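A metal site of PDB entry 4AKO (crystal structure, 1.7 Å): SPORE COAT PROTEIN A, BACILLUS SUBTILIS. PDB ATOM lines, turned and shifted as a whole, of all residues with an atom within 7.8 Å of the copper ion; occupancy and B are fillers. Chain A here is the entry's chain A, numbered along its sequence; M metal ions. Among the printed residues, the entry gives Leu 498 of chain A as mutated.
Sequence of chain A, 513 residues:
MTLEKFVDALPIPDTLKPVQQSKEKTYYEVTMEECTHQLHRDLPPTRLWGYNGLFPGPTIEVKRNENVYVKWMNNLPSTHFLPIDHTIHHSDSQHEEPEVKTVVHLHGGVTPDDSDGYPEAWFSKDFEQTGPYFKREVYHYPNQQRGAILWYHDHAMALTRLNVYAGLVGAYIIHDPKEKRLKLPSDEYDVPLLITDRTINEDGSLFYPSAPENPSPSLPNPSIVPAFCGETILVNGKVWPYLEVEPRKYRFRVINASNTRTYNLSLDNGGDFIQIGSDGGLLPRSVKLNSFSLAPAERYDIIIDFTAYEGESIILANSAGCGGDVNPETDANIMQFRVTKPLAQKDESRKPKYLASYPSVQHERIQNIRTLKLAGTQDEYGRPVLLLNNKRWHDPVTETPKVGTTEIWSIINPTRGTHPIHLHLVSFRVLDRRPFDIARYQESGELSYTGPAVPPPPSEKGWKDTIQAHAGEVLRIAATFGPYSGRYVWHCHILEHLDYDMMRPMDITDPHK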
ATOM      1  N   PRO A 226      10.296  -1.543  24.107  1.00  0.00           N
ATOM      2  CA  PRO A 226      10.741  -0.246  24.640  1.00  0.00           C
ATOM      3  C   PRO A 226      11.754  -0.324  25.798  1.00  0.00           C
ATOM      4  O   PRO A 226      12.245   0.714  26.242  1.00  0.00           O
ATOM      5  CB  PRO A 226       9.443   0.409  25.108  1.00  0.00           C
ATOM      6  CG  PRO A 226       8.551  -0.723  25.451  1.00  0.00           C
ATOM      7  CD  PRO A 226       8.937  -1.894  24.581  1.00  0.00           C
ATOM      8  N   LEU A 374      11.530  15.659  26.129  1.00  0.00           N
ATOM      9  CA  LEU A 374      11.523  14.224  25.891  1.00  0.00           C
ATOM     10  C   LEU A 374      10.078  13.808  25.707  1.00  0.00           C
ATOM     11  O   LEU A 374       9.276  13.877  26.640  1.00  0.00           O
ATOM     12  CB  LEU A 374      12.171  13.480  27.077  1.00  0.00           C
ATOM     13  CG  LEU A 374      13.528  14.016  27.561  1.00  0.00           C
ATOM     14  CD1 LEU A 374      14.065  13.159  28.699  1.00  0.00           C
ATOM     15  CD2 LEU A 374      14.548  14.096  26.421  1.00  0.00           C
ATOM     16  N   LEU A 386       9.627   6.798  20.838  1.00  0.00           N
ATOM     17  CA  LEU A 386      10.197   7.818  21.708  1.00  0.00           C
ATOM     18  C   LEU A 386      10.967   8.836  20.886  1.00  0.00           C
ATOM     19  O   LEU A 386      11.809   8.471  20.062  1.00  0.00           O
ATOM     20  CB  LEU A 386      11.060   7.197  22.802  1.00  0.00           C
ATOM     21  CG  LEU A 386      10.273   6.835  24.068  1.00  0.00           C
ATOM     22  CD1 LEU A 386      10.834   5.599  24.741  1.00  0.00           C
ATOM     23  CD2 LEU A 386      10.214   8.023  25.030  1.00  0.00           C
ATOM     24  N   LEU A 388      12.878  12.886  20.669  1.00  0.00           N
ATOM     25  CA  LEU A 388      13.402  14.128  21.211  1.00  0.00           C
ATOM     26  C   LEU A 388      12.697  15.255  20.462  1.00  0.00           C
ATOM     27  O   LEU A 388      12.742  15.300  19.230  1.00  0.00           O
ATOM     28  CB  LEU A 388      14.915  14.197  21.012  1.00  0.00           C
ATOM     29  CG  LEU A 388      15.747  13.055  21.629  1.00  0.00           C
ATOM     30  CD1 LEU A 388      17.188  13.071  21.122  1.00  0.00           C
ATOM     31  CD2 LEU A 388      15.707  13.116  23.154  1.00  0.00           C
ATOM     32  N   ASN A 413      11.583  16.663  30.968  1.00  0.00           N
ATOM     33  CA  ASN A 413      11.115  15.281  30.961  1.00  0.00           C
ATOM     34  C   ASN A 413       9.720  15.103  31.593  1.00  0.00           C
ATOM     35  O   ASN A 413       9.610  14.924  32.808  1.00  0.00           O
ATOM     36  CB  ASN A 413      12.142  14.348  31.642  1.00  0.00           C
ATOM     37  CG  ASN A 413      11.726  12.885  31.578  1.00  0.00           C
ATOM     38  OD1 ASN A 413      10.727  12.535  30.948  1.00  0.00           O
ATOM     39  ND2 ASN A 413      12.511  12.023  32.206  1.00  0.00           N
ATOM     40  N   THR A 415       7.828  12.517  30.833  1.00  0.00           N
ATOM     41  CA  THR A 415       7.511  11.097  30.727  1.00  0.00           C
ATOM     42  C   THR A 415       7.523  10.423  32.105  1.00  0.00           C
ATOM     43  O   THR A 415       7.831  11.071  33.112  1.00  0.00           O
ATOM     44  CB  THR A 415       8.471  10.338  29.763  1.00  0.00           C
ATOM     45  OG1 THR A 415       9.747  10.174  30.387  1.00  0.00           O
ATOM     46  CG2 THR A 415       8.618  11.096  28.450  1.00  0.00           C
ATOM     47  N   GLY A 417       9.491   7.933  33.154  1.00  0.00           N
ATOM     48  CA  GLY A 417      10.779   7.356  33.560  1.00  0.00           C
ATOM     49  C   GLY A 417      11.974   8.258  33.319  1.00  0.00           C
ATOM     50  O   GLY A 417      11.873   9.275  32.658  1.00  0.00           O
ATOM     51  N   THR A 418      13.107   7.850  33.893  1.00  0.00           N
ATOM     52  CA  THR A 418      14.385   8.533  33.671  1.00  0.00           C
ATOM     53  C   THR A 418      14.943   8.156  32.304  1.00  0.00           C
ATOM     54  O   THR A 418      14.850   7.002  31.868  1.00  0.00           O
ATOM     55  CB  THR A 418      15.412   8.160  34.780  1.00  0.00           C
ATOM     56  OG1 THR A 418      14.926   8.610  36.052  1.00  0.00           O
ATOM     57  CG2 THR A 418      16.766   8.781  34.522  1.00  0.00           C
ATOM     58  N   HIS A 419      15.524   9.134  31.621  1.00  0.00           N
ATOM     59  CA  HIS A 419      16.247   8.884  30.376  1.00  0.00           C
ATOM     60  C   HIS A 419      17.678   9.367  30.561  1.00  0.00           C
ATOM     61  O   HIS A 419      17.885  10.524  30.920  1.00  0.00           O
ATOM     62  CB  HIS A 419      15.583   9.602  29.198  1.00  0.00           C
ATOM     63  CG  HIS A 419      14.174   9.179  28.935  1.00  0.00           C
ATOM     64  ND1 HIS A 419      13.849   8.137  28.097  1.00  0.00           N
ATOM     65  CD2 HIS A 419      12.995   9.652  29.417  1.00  0.00           C
ATOM     66  CE1 HIS A 419      12.535   7.990  28.063  1.00  0.00           C
ATOM     67  NE2 HIS A 419      11.994   8.896  28.855  1.00  0.00           N
ATOM     68  N   PRO A 420      18.660   8.485  30.338  1.00  0.00           N
ATOM     69  CA  PRO A 420      20.060   8.920  30.411  1.00  0.00           C
ATOM     70  C   PRO A 420      20.462   9.568  29.083  1.00  0.00           C
ATOM     71  O   PRO A 420      20.656   8.881  28.088  1.00  0.00           O
ATOM     72  CB  PRO A 420      20.821   7.610  30.666  1.00  0.00           C
ATOM     73  CG  PRO A 420      19.993   6.569  29.999  1.00  0.00           C
ATOM     74  CD  PRO A 420      18.551   7.044  30.054  1.00  0.00           C
ATOM     75  N   ILE A 421      20.542  10.901  29.076  1.00  0.00           N
ATOM     76  CA  ILE A 421      20.825  11.654  27.858  1.00  0.00           C
ATOM     77  C   ILE A 421      22.321  11.818  27.617  1.00  0.00           C
ATOM     78  O   ILE A 421      23.068  12.254  28.499  1.00  0.00           O
ATOM     79  CB  ILE A 421      20.073  13.026  27.855  1.00  0.00           C
ATOM     80  CG1 ILE A 421      18.580  12.834  28.138  1.00  0.00           C
ATOM     81  CG2 ILE A 421      20.321  13.797  26.542  1.00  0.00           C
ATOM     82  CD1 ILE A 421      17.810  12.068  27.052  1.00  0.00           C
ATOM     83  N   HIS A 491      21.294  11.833  22.118  1.00  0.00           N
ATOM     84  CA  HIS A 491      20.266  10.796  22.245  1.00  0.00           C
ATOM     85  C   HIS A 491      20.137  10.259  23.655  1.00  0.00           C
ATOM     86  O   HIS A 491      20.973  10.495  24.520  1.00  0.00           O
ATOM     87  CB  HIS A 491      20.584   9.626  21.298  1.00  0.00           C
ATOM     88  CG  HIS A 491      21.911   8.975  21.550  1.00  0.00           C
ATOM     89  ND1 HIS A 491      22.081   7.931  22.435  1.00  0.00           N
ATOM     90  CD2 HIS A 491      23.136   9.216  21.019  1.00  0.00           C
ATOM     91  CE1 HIS A 491      23.344   7.563  22.454  1.00  0.00           C
ATOM     92  NE2 HIS A 491      24.008   8.318  21.595  1.00  0.00           N
ATOM     93  N   CYS A 492      19.057   9.524  23.877  1.00  0.00           N
ATOM     94  CA  CYS A 492      18.920   8.712  25.066  1.00  0.00           C
ATOM     95  C   CYS A 492      19.778   7.464  24.902  1.00  0.00           C
ATOM     96  O   CYS A 492      19.824   6.890  23.802  1.00  0.00           O
ATOM     97  CB  CYS A 492      17.461   8.328  25.261  1.00  0.00           C
ATOM     98  SG  CYS A 492      17.242   7.246  26.641  1.00  0.00           S
ATOM     99  N   HIS A 493      20.468   7.047  25.969  1.00  0.00           N
ATOM    100  CA  HIS A 493      21.330   5.858  25.910  1.00  0.00           C
ATOM    101  C   HIS A 493      20.651   4.569  26.410  1.00  0.00           C
ATOM    102  O   HIS A 493      21.305   3.539  26.617  1.00  0.00           O
ATOM    103  CB  HIS A 493      22.701   6.104  26.598  1.00  0.00           C
ATOM    104  CG  HIS A 493      23.872   5.448  25.913  1.00  0.00           C
ATOM    105  ND1 HIS A 493      24.086   4.086  25.923  1.00  0.00           N
ATOM    106  CD2 HIS A 493      24.927   5.983  25.232  1.00  0.00           C
ATOM    107  CE1 HIS A 493      25.194   3.806  25.264  1.00  0.00           C
ATOM    108  NE2 HIS A 493      25.731   4.939  24.835  1.00  0.00           N
ATOM    109  N   ILE A 494      19.331   4.614  26.598  1.00  0.00           N
ATOM    110  CA  ILE A 494      18.555   3.380  26.673  1.00  0.00           C
ATOM    111  C   ILE A 494      18.430   2.924  25.217  1.00  0.00           C
ATOM    112  O   ILE A 494      17.773   3.578  24.411  1.00  0.00           O
ATOM    113  CB  ILE A 494      17.164   3.539  27.347  1.00  0.00           C
ATOM    114  CG1 ILE A 494      17.342   3.823  28.842  1.00  0.00           C
ATOM    115  CG2 ILE A 494      16.321   2.267  27.146  1.00  0.00           C
ATOM    116  CD1 ILE A 494      16.080   4.307  29.533  1.00  0.00           C
ATOM    117  N   LEU A 495      19.103   1.829  24.891  1.00  0.00           N
ATOM    118  CA  LEU A 495      19.289   1.485  23.484  1.00  0.00           C
ATOM    119  C   LEU A 495      17.981   1.166  22.768  1.00  0.00           C
ATOM    120  O   LEU A 495      17.834   1.448  21.579  1.00  0.00           O
ATOM    121  CB  LEU A 495      20.309   0.349  23.327  1.00  0.00           C
ATOM    122  CG  LEU A 495      21.694   0.661  23.907  1.00  0.00           C
ATOM    123  CD1 LEU A 495      22.650  -0.490  23.601  1.00  0.00           C
ATOM    124  CD2 LEU A 495      22.270   1.987  23.376  1.00  0.00           C
ATOM    125  N   GLU A 496      17.034   0.609  23.512  1.00  0.00           N
ATOM    126  CA  GLU A 496      15.690   0.342  23.004  1.00  0.00           C
ATOM    127  C   GLU A 496      14.936   1.634  22.651  1.00  0.00           C
ATOM    128  O   GLU A 496      14.037   1.615  21.801  1.00  0.00           O
ATOM    129  CB  GLU A 496      14.907  -0.477  24.019  1.00  0.00           C
ATOM    130  CG  GLU A 496      15.274  -1.969  24.060  1.00  0.00           C
ATOM    131  CD  GLU A 496      16.649  -2.270  24.653  1.00  0.00           C
ATOM    132  OE1 GLU A 496      17.171  -1.466  25.456  1.00  0.00           O
ATOM    133  OE2 GLU A 496      17.217  -3.335  24.308  1.00  0.00           O
ATOM    134  N   HIS A 497      15.299   2.738  23.310  1.00  0.00           N
ATOM    135  CA  HIS A 497      14.739   4.068  23.010  1.00  0.00           C
ATOM    136  C   HIS A 497      15.475   4.697  21.837  1.00  0.00           C
ATOM    137  O   HIS A 497      14.861   5.206  20.906  1.00  0.00           O
ATOM    138  CB  HIS A 497      14.842   5.001  24.222  1.00  0.00           C
ATOM    139  CG  HIS A 497      14.039   4.560  25.410  1.00  0.00           C
ATOM    140  ND1 HIS A 497      13.951   5.313  26.557  1.00  0.00           N
ATOM    141  CD2 HIS A 497      13.265   3.465  25.607  1.00  0.00           C
ATOM    142  CE1 HIS A 497      13.174   4.683  27.431  1.00  0.00           C
ATOM    143  NE2 HIS A 497      12.745   3.556  26.877  1.00  0.00           N
ATOM    144  N   LEU A 498      16.806   4.664  21.908  1.00  0.00           N
ATOM    145  CA  LEU A 498      17.676   5.176  20.859  1.00  0.00           C
ATOM    146  C   LEU A 498      17.231   4.705  19.468  1.00  0.00           C
ATOM    147  O   LEU A 498      17.076   5.517  18.560  1.00  0.00           O
ATOM    148  CB  LEU A 498      19.134   4.756  21.143  1.00  0.00           C
ATOM    149  CG  LEU A 498      20.310   5.327  20.350  1.00  0.00           C
ATOM    150  CD1 LEU A 498      21.587   4.915  21.060  1.00  0.00           C
ATOM    151  CD2 LEU A 498      20.338   4.849  18.909  1.00  0.00           C
ATOM    152  N   MET A 502      14.737   7.778  19.585  1.00  0.00           N
ATOM    153  CA  MET A 502      15.110   8.850  20.513  1.00  0.00           C
ATOM    154  C   MET A 502      16.541   9.346  20.307  1.00  0.00           C
ATOM    155  O   MET A 502      17.356   9.366  21.239  1.00  0.00           O
ATOM    156  CB  MET A 502      14.851   8.405  21.957  1.00  0.00           C
ATOM    157  CG  MET A 502      14.614   9.541  22.925  1.00  0.00           C
ATOM    158  SD  MET A 502      14.037   8.896  24.490  1.00  0.00           S
ATOM    159  CE  MET A 502      13.862  10.395  25.434  1.00  0.00           C
HETATM  160 CU    CU M   1      14.992   6.975  26.935  1.00  0.00          CU
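O of His 497 is in hydrogen-bond range of N of Met 502, 2.9 Å away.
A ring nitrogen (NE2) of His 497 lies within hydrogen-bond range of the backbone carbonyl oxygen (O) of Pro 226 (3.0 Å).
A ring nitrogen (ND1) of His 419 sits close to the side-chain sulfur (SD) of Met 502, 3.7 Å away.
NE2 of His 419 is in hydrogen-bond range of OG1 of Thr 415, at 3.0 Å.
N of Cys 492 lies within hydrogen-bond range of O of Met 502, 3.1 Å away.
SG of Cys 492 sits close to N of Ile 494.
N of Met 502 is in hydrogen-bond range of O of Leu 386, 3.0 Å away.
Ile 494 touches the copper ion.
Met 502 touches the copper ion (SD to CU, 3.3 Å).
Of the 20 residues printed, 5 come within 4 Å of the copper ion.
ND1 of His 497 is bound to the copper ion (2.0 Å).
A ring nitrogen (ND1) of His 419 binds the copper ion, at 2.0 Å.
The copper ion is bound by SG of Cys 492 (2.3 Å).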
